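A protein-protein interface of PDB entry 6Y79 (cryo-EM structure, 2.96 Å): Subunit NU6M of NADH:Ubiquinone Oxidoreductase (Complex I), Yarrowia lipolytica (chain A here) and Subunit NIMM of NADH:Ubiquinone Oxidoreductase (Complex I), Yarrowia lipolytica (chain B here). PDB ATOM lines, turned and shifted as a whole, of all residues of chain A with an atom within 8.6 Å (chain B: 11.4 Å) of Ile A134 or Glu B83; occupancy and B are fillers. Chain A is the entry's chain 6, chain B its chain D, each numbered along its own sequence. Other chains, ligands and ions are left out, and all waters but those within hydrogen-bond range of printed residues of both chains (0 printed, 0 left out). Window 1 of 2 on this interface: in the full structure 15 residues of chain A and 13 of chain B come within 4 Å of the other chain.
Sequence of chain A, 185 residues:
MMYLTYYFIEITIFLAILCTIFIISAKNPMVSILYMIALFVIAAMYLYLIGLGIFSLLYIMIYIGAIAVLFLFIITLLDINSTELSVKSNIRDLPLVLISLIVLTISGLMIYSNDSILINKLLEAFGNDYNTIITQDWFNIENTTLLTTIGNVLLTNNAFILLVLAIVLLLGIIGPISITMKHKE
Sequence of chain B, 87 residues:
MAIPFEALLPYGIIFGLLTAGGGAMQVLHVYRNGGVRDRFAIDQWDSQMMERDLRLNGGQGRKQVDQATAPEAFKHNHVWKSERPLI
Of chain B, only Lys B81 and Glu B83 come within 4 Å of Ile A134. Of the printed residues of chain B, Asn A131 touches Glu B83, Arg B84 and Pro B85. Thr A132 touches just these residues of chain B: Lys B81 (3.6 Å), Ser B82 (3.3 Å) and Glu B83 (2.9 Å). Of the printed residues of chain B, Ile A133 touches Trp B80 and Lys B81. No residue of chain B comes within 4 Å of Thr A135. Ser B82 touches just one residue of chain A: Thr A132. Printed residues of chain A within 4 Å of Glu B51: Gln A136. Printed residues of chain A within 4 Å of Lys B81: Thr A132 (3.6 Å), Ile A133 (3.6 Å) and Ile A134 (2.7 Å). Of the printed residues of chain B, Asp A137 touches Gln B48 (3.8 Å). Of the printed residues of chain A, Ile B87 touches Ile A9 (3.8 Å). Printed residues of chain A within 4 Å of Arg B84: Tyr A6 (3.0 Å), Ile A9 (3.4 Å) and Asn A131 (3.4 Å). Asp A129 touches none of the printed residues of chain B. The nearest printed residue of chain B that does not touch Tyr A6 is Ile B87 (5.7 Å).
Of the 13 printed residues of chain B, 10 touch a printed residue of chain A. Printed residues of chain A that touch a printed residue of chain B: Tyr A6, Ile A9, Ile A50, Asn A128, Asn A131, Thr A132, Ile A133, Ile A134, Gln A136 and Asp A137. Among the printed residues, 19 pairs touch across the chains.
The side-chain carboxylate (OE1) of Glu B51 lies within salt-bridge range of the side-chain amino group (NZ) of Lys B81 (3.2 Å).
The backbone NH (N) of Glu B83 sits at hydrogen-bond distance from the backbone carbonyl oxygen (O) of Thr A132, 2.9 Å away. The backbone carbonyl oxygen (O) of Tyr A6 is in hydrogen-bond range of the guanidinium group (NE) of Arg B84 (3.0 Å). O of Lys B81 is in hydrogen-bond range of N of Ile A134 (2.7 Å). The side-chain amide nitrogen of Gln A136 lies within hydrogen-bond range of the side-chain carboxylate of Glu B51 (2.7 Å).
Tyr A6 touches Pro B85 (OH to CD, 3.8 Å). Ile A9 touches Arg B84 (CD1 to NH1, 3.4 Å). Ile A50 touches Leu B86 (CG1 to CD2, 3.7 Å). Asn A128 touches Pro B85 (O to CB, 3.3 Å). Asn A131 touches Glu B83. CD of Pro B85 touches OD1 of Asn A131, 3.3 Å away. Ile A133 touches Trp B80 (CG2 to CE3, 3.6 Å). Lys B81 touches Ile A133 (O to C, 3.6 Å). Ile A134 touches Glu B83. Asp A137 touches Gln B48 (O to OE1, 3.8 Å).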
ATOM      1  N   TYR A   6      -4.226   6.596   8.102  1.00  0.00           N
ATOM      2  CA  TYR A   6      -2.820   6.688   7.739  1.00  0.00           C
ATOM      3  C   TYR A   6      -2.414   8.129   7.468  1.00  0.00           C
ATOM      4  O   TYR A   6      -1.368   8.591   7.932  1.00  0.00           O
ATOM      5  CB  TYR A   6      -2.570   5.809   6.510  1.00  0.00           C
ATOM      6  CG  TYR A   6      -1.211   5.935   5.882  1.00  0.00           C
ATOM      7  CD1 TYR A   6      -0.129   5.232   6.383  1.00  0.00           C
ATOM      8  CD2 TYR A   6      -1.013   6.738   4.769  1.00  0.00           C
ATOM      9  CE1 TYR A   6       1.113   5.341   5.808  1.00  0.00           C
ATOM     10  CE2 TYR A   6       0.222   6.859   4.193  1.00  0.00           C
ATOM     11  CZ  TYR A   6       1.280   6.155   4.715  1.00  0.00           C
ATOM     12  OH  TYR A   6       2.516   6.266   4.137  1.00  0.00           O
ATOM     13  N   ILE A   9      -1.213  12.912   9.355  1.00  0.00           N
ATOM     14  CA  ILE A   9      -0.191  13.949   9.377  1.00  0.00           C
ATOM     15  C   ILE A   9      -0.311  14.852   8.158  1.00  0.00           C
ATOM     16  O   ILE A   9      -0.225  16.082   8.270  1.00  0.00           O
ATOM     17  CB  ILE A   9       1.192  13.286   9.479  1.00  0.00           C
ATOM     18  CG1 ILE A   9       1.302  12.563  10.820  1.00  0.00           C
ATOM     19  CG2 ILE A   9       2.312  14.294   9.292  1.00  0.00           C
ATOM     20  CD1 ILE A   9       2.652  12.041  11.135  1.00  0.00           C
ATOM     21  N   LEU A  49      -0.116  13.642  17.584  1.00  0.00           N
ATOM     22  CA  LEU A  49      -0.013  12.705  16.477  1.00  0.00           C
ATOM     23  C   LEU A  49       1.383  12.109  16.371  1.00  0.00           C
ATOM     24  O   LEU A  49       1.532  10.904  16.166  1.00  0.00           O
ATOM     25  CB  LEU A  49      -0.389  13.445  15.200  1.00  0.00           C
ATOM     26  CG  LEU A  49      -0.818  12.751  13.927  1.00  0.00           C
ATOM     27  CD1 LEU A  49      -1.836  11.699  14.253  1.00  0.00           C
ATOM     28  CD2 LEU A  49      -1.419  13.811  13.035  1.00  0.00           C
ATOM     29  N   ILE A  50       2.416  12.930  16.546  1.00  0.00           N
ATOM     30  CA  ILE A  50       3.785  12.445  16.420  1.00  0.00           C
ATOM     31  C   ILE A  50       4.225  11.642  17.646  1.00  0.00           C
ATOM     32  O   ILE A  50       5.120  10.797  17.540  1.00  0.00           O
ATOM     33  CB  ILE A  50       4.700  13.648  16.119  1.00  0.00           C
ATOM     34  CG1 ILE A  50       6.091  13.208  15.695  1.00  0.00           C
ATOM     35  CG2 ILE A  50       4.808  14.583  17.293  1.00  0.00           C
ATOM     36  CD1 ILE A  50       6.909  14.314  15.165  1.00  0.00           C
ATOM     37  N   GLY A  51       3.590  11.838  18.796  1.00  0.00           N
ATOM     38  CA  GLY A  51       3.908  11.039  19.962  1.00  0.00           C
ATOM     39  C   GLY A  51       4.137  11.852  21.216  1.00  0.00           C
ATOM     40  O   GLY A  51       4.427  11.300  22.277  1.00  0.00           O
ATOM     41  N   ASN A 128      11.251   9.793   1.664  1.00  0.00           N
ATOM     42  CA  ASN A 128      10.641   9.642   2.971  1.00  0.00           C
ATOM     43  C   ASN A 128      10.071   8.256   3.213  1.00  0.00           C
ATOM     44  O   ASN A 128       9.894   7.876   4.371  1.00  0.00           O
ATOM     45  CB  ASN A 128       9.497  10.647   3.135  1.00  0.00           C
ATOM     46  CG  ASN A 128       9.969  12.073   3.146  1.00  0.00           C
ATOM     47  OD1 ASN A 128      10.939  12.418   3.822  1.00  0.00           O
ATOM     48  ND2 ASN A 128       9.290  12.918   2.384  1.00  0.00           N
ATOM     49  N   ASP A 129       9.817   7.485   2.166  1.00  0.00           N
ATOM     50  CA  ASP A 129       8.891   6.364   2.033  1.00  0.00           C
ATOM     51  C   ASP A 129       9.167   5.173   3.013  1.00  0.00           C
ATOM     52  O   ASP A 129       8.346   4.254   3.158  1.00  0.00           O
ATOM     53  CB  ASP A 129       8.955   5.911   0.575  1.00  0.00           C
ATOM     54  CG  ASP A 129       7.943   4.837   0.243  1.00  0.00           C
ATOM     55  OD1 ASP A 129       6.762   4.997   0.611  1.00  0.00           O
ATOM     56  OD2 ASP A 129       8.340   3.833  -0.380  1.00  0.00           O
ATOM     57  N   TYR A 130      10.228   5.113   3.799  1.00  0.00           N
ATOM     58  CA  TYR A 130      10.579   3.874   4.470  1.00  0.00           C
ATOM     59  C   TYR A 130      10.078   3.888   5.905  1.00  0.00           C
ATOM     60  O   TYR A 130      10.203   4.893   6.608  1.00  0.00           O
ATOM     61  CB  TYR A 130      12.082   3.656   4.355  1.00  0.00           C
ATOM     62  CG  TYR A 130      12.383   3.425   2.902  1.00  0.00           C
ATOM     63  CD1 TYR A 130      12.091   2.207   2.316  1.00  0.00           C
ATOM     64  CD2 TYR A 130      12.857   4.451   2.092  1.00  0.00           C
ATOM     65  CE1 TYR A 130      12.312   1.993   0.988  1.00  0.00           C
ATOM     66  CE2 TYR A 130      13.078   4.247   0.759  1.00  0.00           C
ATOM     67  CZ  TYR A 130      12.802   3.015   0.214  1.00  0.00           C
ATOM     68  OH  TYR A 130      13.010   2.805  -1.118  1.00  0.00           O
ATOM     69  N   ASN A 131       9.471   2.778   6.316  1.00  0.00           N
ATOM     70  CA  ASN A 131       8.701   2.708   7.551  1.00  0.00           C
ATOM     71  C   ASN A 131       9.615   2.250   8.676  1.00  0.00           C
ATOM     72  O   ASN A 131      10.134   1.134   8.630  1.00  0.00           O
ATOM     73  CB  ASN A 131       7.522   1.754   7.391  1.00  0.00           C
ATOM     74  CG  ASN A 131       6.289   2.439   6.882  1.00  0.00           C
ATOM     75  OD1 ASN A 131       6.355   3.543   6.357  1.00  0.00           O
ATOM     76  ND2 ASN A 131       5.145   1.794   7.052  1.00  0.00           N
ATOM     77  N   THR A 132       9.798   3.100   9.688  1.00  0.00           N
ATOM     78  CA  THR A 132      10.731   2.805  10.768  1.00  0.00           C
ATOM     79  C   THR A 132      10.272   1.595  11.577  1.00  0.00           C
ATOM     80  O   THR A 132       9.080   1.395  11.808  1.00  0.00           O
ATOM     81  CB  THR A 132      10.933   4.048  11.661  1.00  0.00           C
ATOM     82  OG1 THR A 132      11.886   3.766  12.693  1.00  0.00           O
ATOM     83  CG2 THR A 132       9.642   4.563  12.267  1.00  0.00           C
ATOM     84  N   ILE A 133      11.221   0.734  11.916  1.00  0.00           N
ATOM     85  CA  ILE A 133      10.936  -0.478  12.673  1.00  0.00           C
ATOM     86  C   ILE A 133      11.118  -0.163  14.149  1.00  0.00           C
ATOM     87  O   ILE A 133      12.201   0.256  14.572  1.00  0.00           O
ATOM     88  CB  ILE A 133      11.845  -1.637  12.239  1.00  0.00           C
ATOM     89  CG1 ILE A 133      11.499  -2.081  10.822  1.00  0.00           C
ATOM     90  CG2 ILE A 133      11.721  -2.793  13.201  1.00  0.00           C
ATOM     91  CD1 ILE A 133      12.339  -3.227  10.319  1.00  0.00           C
ATOM     92  N   ILE A 134      10.065  -0.358  14.935  1.00  0.00           N
ATOM     93  CA  ILE A 134      10.099  -0.104  16.369  1.00  0.00           C
ATOM     94  C   ILE A 134      10.294  -1.433  17.087  1.00  0.00           C
ATOM     95  O   ILE A 134       9.502  -2.365  16.913  1.00  0.00           O
ATOM     96  CB  ILE A 134       8.826   0.607  16.847  1.00  0.00           C
ATOM     97  CG1 ILE A 134       8.728   1.998  16.228  1.00  0.00           C
ATOM     98  CG2 ILE A 134       8.826   0.720  18.349  1.00  0.00           C
ATOM     99  CD1 ILE A 134       9.883   2.898  16.583  1.00  0.00           C
ATOM    100  N   THR A 135      11.350  -1.510  17.888  1.00  0.00           N
ATOM    101  CA  THR A 135      11.751  -2.692  18.633  1.00  0.00           C
ATOM    102  C   THR A 135      11.457  -2.449  20.109  1.00  0.00           C
ATOM    103  O   THR A 135      11.472  -1.305  20.572  1.00  0.00           O
ATOM    104  CB  THR A 135      13.250  -2.968  18.365  1.00  0.00           C
ATOM    105  OG1 THR A 135      13.409  -3.456  17.027  1.00  0.00           O
ATOM    106  CG2 THR A 135      13.917  -3.970  19.331  1.00  0.00           C
ATOM    107  N   GLN A 136      11.133  -3.509  20.846  1.00  0.00           N
ATOM    108  CA  GLN A 136      11.024  -3.416  22.293  1.00  0.00           C
ATOM    109  C   GLN A 136      12.301  -3.892  22.952  1.00  0.00           C
ATOM    110  O   GLN A 136      12.782  -4.993  22.674  1.00  0.00           O
ATOM    111  CB  GLN A 136       9.873  -4.253  22.794  1.00  0.00           C
ATOM    112  CG  GLN A 136       8.644  -3.826  22.167  1.00  0.00           C
ATOM    113  CD  GLN A 136       7.579  -4.821  22.424  1.00  0.00           C
ATOM    114  OE1 GLN A 136       7.766  -5.765  23.182  1.00  0.00           O
ATOM    115  NE2 GLN A 136       6.491  -4.722  21.681  1.00  0.00           N
ATOM    116  N   ASP A 137      12.842  -3.068  23.824  1.00  0.00           N
ATOM    117  CA  ASP A 137      13.897  -3.482  24.724  1.00  0.00           C
ATOM    118  C   ASP A 137      13.435  -3.222  26.147  1.00  0.00           C
ATOM    119  O   ASP A 137      12.777  -2.214  26.417  1.00  0.00           O
ATOM    120  CB  ASP A 137      15.192  -2.746  24.406  1.00  0.00           C
ATOM    121  CG  ASP A 137      15.029  -1.257  24.458  1.00  0.00           C
ATOM    122  OD1 ASP A 137      14.270  -0.716  23.628  1.00  0.00           O
ATOM    123  OD2 ASP A 137      15.655  -0.623  25.326  1.00  0.00           O
ATOM    124  N   GLN B  44       5.239   2.395  30.796  1.00  0.00           N
ATOM    125  CA  GLN B  44       5.706   1.853  29.525  1.00  0.00           C
ATOM    126  C   GLN B  44       6.069   0.382  29.680  1.00  0.00           C
ATOM    127  O   GLN B  44       5.775  -0.445  28.806  1.00  0.00           O
ATOM    128  CB  GLN B  44       6.899   2.664  29.020  1.00  0.00           C
ATOM    129  CG  GLN B  44       7.678   2.045  27.862  1.00  0.00           C
ATOM    130  CD  GLN B  44       8.820   2.928  27.405  1.00  0.00           C
ATOM    131  OE1 GLN B  44       9.173   3.893  28.078  1.00  0.00           O
ATOM    132  NE2 GLN B  44       9.414   2.598  26.267  1.00  0.00           N
ATOM    133  N   GLN B  48       4.234  -2.781  27.833  1.00  0.00           N
ATOM    134  CA  GLN B  48       4.939  -3.862  27.147  1.00  0.00           C
ATOM    135  C   GLN B  48       4.634  -5.211  27.780  1.00  0.00           C
ATOM    136  O   GLN B  48       4.618  -6.249  27.110  1.00  0.00           O
ATOM    137  CB  GLN B  48       6.435  -3.593  27.158  1.00  0.00           C
ATOM    138  CG  GLN B  48       6.866  -2.460  26.282  1.00  0.00           C
ATOM    139  CD  GLN B  48       8.351  -2.242  26.344  1.00  0.00           C
ATOM    140  OE1 GLN B  48       9.057  -2.926  27.075  1.00  0.00           O
ATOM    141  NE2 GLN B  48       8.837  -1.285  25.575  1.00  0.00           N
ATOM    142  N   GLU B  51       1.071  -6.310  26.468  1.00  0.00           N
ATOM    143  CA  GLU B  51       1.097  -6.856  25.108  1.00  0.00           C
ATOM    144  C   GLU B  51       1.817  -8.202  25.058  1.00  0.00           C
ATOM    145  O   GLU B  51       1.441  -9.077  24.266  1.00  0.00           O
ATOM    146  CB  GLU B  51       1.708  -5.856  24.127  1.00  0.00           C
ATOM    147  CG  GLU B  51       3.168  -5.659  24.332  1.00  0.00           C
ATOM    148  CD  GLU B  51       3.795  -4.545  23.582  1.00  0.00           C
ATOM    149  OE1 GLU B  51       3.145  -3.801  22.795  1.00  0.00           O
ATOM    150  OE2 GLU B  51       5.015  -4.304  23.860  1.00  0.00           O
ATOM    151  N   HIS B  78       5.517 -13.344  17.385  1.00  0.00           N
ATOM    152  CA  HIS B  78       6.122 -12.135  17.921  1.00  0.00           C
ATOM    153  C   HIS B  78       5.994 -10.973  16.947  1.00  0.00           C
ATOM    154  O   HIS B  78       6.098 -11.149  15.740  1.00  0.00           O
ATOM    155  CB  HIS B  78       7.593 -12.370  18.246  1.00  0.00           C
ATOM    156  CG  HIS B  78       8.298 -11.131  18.681  1.00  0.00           C
ATOM    157  ND1 HIS B  78       7.907 -10.415  19.789  1.00  0.00           N
ATOM    158  CD2 HIS B  78       9.313 -10.436  18.121  1.00  0.00           C
ATOM    159  CE1 HIS B  78       8.679  -9.352  19.916  1.00  0.00           C
ATOM    160  NE2 HIS B  78       9.542  -9.343  18.919  1.00  0.00           N
ATOM    161  N   VAL B  79       5.814  -9.776  17.484  1.00  0.00           N
ATOM    162  CA  VAL B  79       5.444  -8.591  16.724  1.00  0.00           C
ATOM    163  C   VAL B  79       6.562  -7.553  16.788  1.00  0.00           C
ATOM    164  O   VAL B  79       7.167  -7.340  17.843  1.00  0.00           O
ATOM    165  CB  VAL B  79       4.112  -8.053  17.285  1.00  0.00           C
ATOM    166  CG1 VAL B  79       3.910  -6.594  16.989  1.00  0.00           C
ATOM    167  CG2 VAL B  79       2.969  -8.873  16.750  1.00  0.00           C
ATOM    168  N   TRP B  80       6.867  -6.948  15.642  1.00  0.00           N
ATOM    169  CA  TRP B  80       7.479  -5.633  15.565  1.00  0.00           C
ATOM    170  C   TRP B  80       6.434  -4.649  15.063  1.00  0.00           C
ATOM    171  O   TRP B  80       5.434  -5.031  14.454  1.00  0.00           O
ATOM    172  CB  TRP B  80       8.669  -5.609  14.611  1.00  0.00           C
ATOM    173  CG  TRP B  80       9.899  -6.255  15.073  1.00  0.00           C
ATOM    174  CD1 TRP B  80      10.179  -6.697  16.322  1.00  0.00           C
ATOM    175  CD2 TRP B  80      11.044  -6.543  14.273  1.00  0.00           C
ATOM    176  NE1 TRP B  80      11.438  -7.242  16.356  1.00  0.00           N
ATOM    177  CE2 TRP B  80      11.989  -7.160  15.106  1.00  0.00           C
ATOM    178  CE3 TRP B  80      11.360  -6.340  12.928  1.00  0.00           C
ATOM    179  CZ2 TRP B  80      13.229  -7.575  14.639  1.00  0.00           C
ATOM    180  CZ3 TRP B  80      12.590  -6.743  12.470  1.00  0.00           C
ATOM    181  CH2 TRP B  80      13.510  -7.357  13.321  1.00  0.00           C
ATOM    182  N   LYS B  81       6.676  -3.371  15.306  1.00  0.00           N
ATOM    183  CA  LYS B  81       5.771  -2.317  14.878  1.00  0.00           C
ATOM    184  C   LYS B  81       6.480  -1.467  13.835  1.00  0.00           C
ATOM    185  O   LYS B  81       7.555  -0.926  14.103  1.00  0.00           O
ATOM    186  CB  LYS B  81       5.327  -1.474  16.070  1.00  0.00           C
ATOM    187  CG  LYS B  81       4.929  -2.312  17.267  1.00  0.00           C
ATOM    188  CD  LYS B  81       4.422  -1.461  18.402  1.00  0.00           C
ATOM    189  CE  LYS B  81       3.643  -2.301  19.389  1.00  0.00           C
ATOM    190  NZ  LYS B  81       3.235  -1.531  20.589  1.00  0.00           N
ATOM    191  N   SER B  82       5.896  -1.378  12.645  1.00  0.00           N
ATOM    192  CA  SER B  82       6.433  -0.565  11.561  1.00  0.00           C
ATOM    193  C   SER B  82       5.623   0.720  11.475  1.00  0.00           C
ATOM    194  O   SER B  82       4.458   0.706  11.070  1.00  0.00           O
ATOM    195  CB  SER B  82       6.394  -1.317  10.237  1.00  0.00           C
ATOM    196  OG  SER B  82       5.063  -1.517   9.814  1.00  0.00           O
ATOM    197  N   GLU B  83       6.255   1.824  11.845  1.00  0.00           N
ATOM    198  CA  GLU B  83       5.636   3.136  11.881  1.00  0.00           C
ATOM    199  C   GLU B  83       5.948   3.907  10.605  1.00  0.00           C
ATOM    200  O   GLU B  83       7.070   3.867  10.107  1.00  0.00           O
ATOM    201  CB  GLU B  83       6.134   3.883  13.118  1.00  0.00           C
ATOM    202  CG  GLU B  83       5.833   5.357  13.168  1.00  0.00           C
ATOM    203  CD  GLU B  83       6.232   5.997  14.463  1.00  0.00           C
ATOM    204  OE1 GLU B  83       6.846   5.321  15.315  1.00  0.00           O
ATOM    205  OE2 GLU B  83       5.895   7.174  14.656  1.00  0.00           O
ATOM    206  N   ARG B  84       4.953   4.644  10.108  1.00  0.00           N
ATOM    207  CA  ARG B  84       4.872   5.389   8.854  1.00  0.00           C
ATOM    208  C   ARG B  84       5.937   6.495   8.735  1.00  0.00           C
ATOM    209  O   ARG B  84       6.636   6.751   9.724  1.00  0.00           O
ATOM    210  CB  ARG B  84       3.436   5.917   8.776  1.00  0.00           C
ATOM    211  CG  ARG B  84       3.171   7.133   9.573  1.00  0.00           C
ATOM    212  CD  ARG B  84       1.734   7.512   9.365  1.00  0.00           C
ATOM    213  NE  ARG B  84       1.552   7.910   7.985  1.00  0.00           N
ATOM    214  CZ  ARG B  84       1.698   9.153   7.558  1.00  0.00           C
ATOM    215  NH1 ARG B  84       1.996  10.113   8.411  1.00  0.00           N
ATOM    216  NH2 ARG B  84       1.533   9.433   6.281  1.00  0.00           N
ATOM    217  N   PRO B  85       6.127   7.138   7.556  1.00  0.00           N
ATOM    218  CA  PRO B  85       7.276   8.056   7.382  1.00  0.00           C
ATOM    219  C   PRO B  85       7.387   9.263   8.307  1.00  0.00           C
ATOM    220  O   PRO B  85       8.489   9.821   8.376  1.00  0.00           O
ATOM    221  CB  PRO B  85       7.094   8.537   5.939  1.00  0.00           C
ATOM    222  CG  PRO B  85       6.573   7.398   5.268  1.00  0.00           C
ATOM    223  CD  PRO B  85       5.622   6.754   6.218  1.00  0.00           C
ATOM    224  N   LEU B  86       6.309   9.691   8.976  1.00  0.00           N
ATOM    225  CA  LEU B  86       6.268  10.891   9.827  1.00  0.00           C
ATOM    226  C   LEU B  86       6.635  12.147   9.027  1.00  0.00           C
ATOM    227  O   LEU B  86       7.604  12.850   9.313  1.00  0.00           O
ATOM    228  CB  LEU B  86       7.161  10.726  11.067  1.00  0.00           C
ATOM    229  CG  LEU B  86       6.784  11.292  12.434  1.00  0.00           C
ATOM    230  CD1 LEU B  86       5.511  10.696  12.942  1.00  0.00           C
ATOM    231  CD2 LEU B  86       7.860  10.919  13.382  1.00  0.00           C
ATOM    232  N   ILE B  87       5.830  12.399   8.001  1.00  0.00           N
ATOM    233  CA  ILE B  87       5.992  13.506   7.078  1.00  0.00           C
ATOM    234  C   ILE B  87       5.751  14.852   7.766  1.00  0.00           C
ATOM    235  O   ILE B  87       6.654  15.689   7.890  1.00  0.00           O
ATOM    236  CB  ILE B  87       5.055  13.296   5.866  1.00  0.00           C
ATOM    237  CG1 ILE B  87       5.351  11.939   5.198  1.00  0.00           C
ATOM    238  CG2 ILE B  87       5.162  14.432   4.874  1.00  0.00           C
ATOM    239  CD1 ILE B  87       4.455  11.589   4.012  1.00  0.00           C
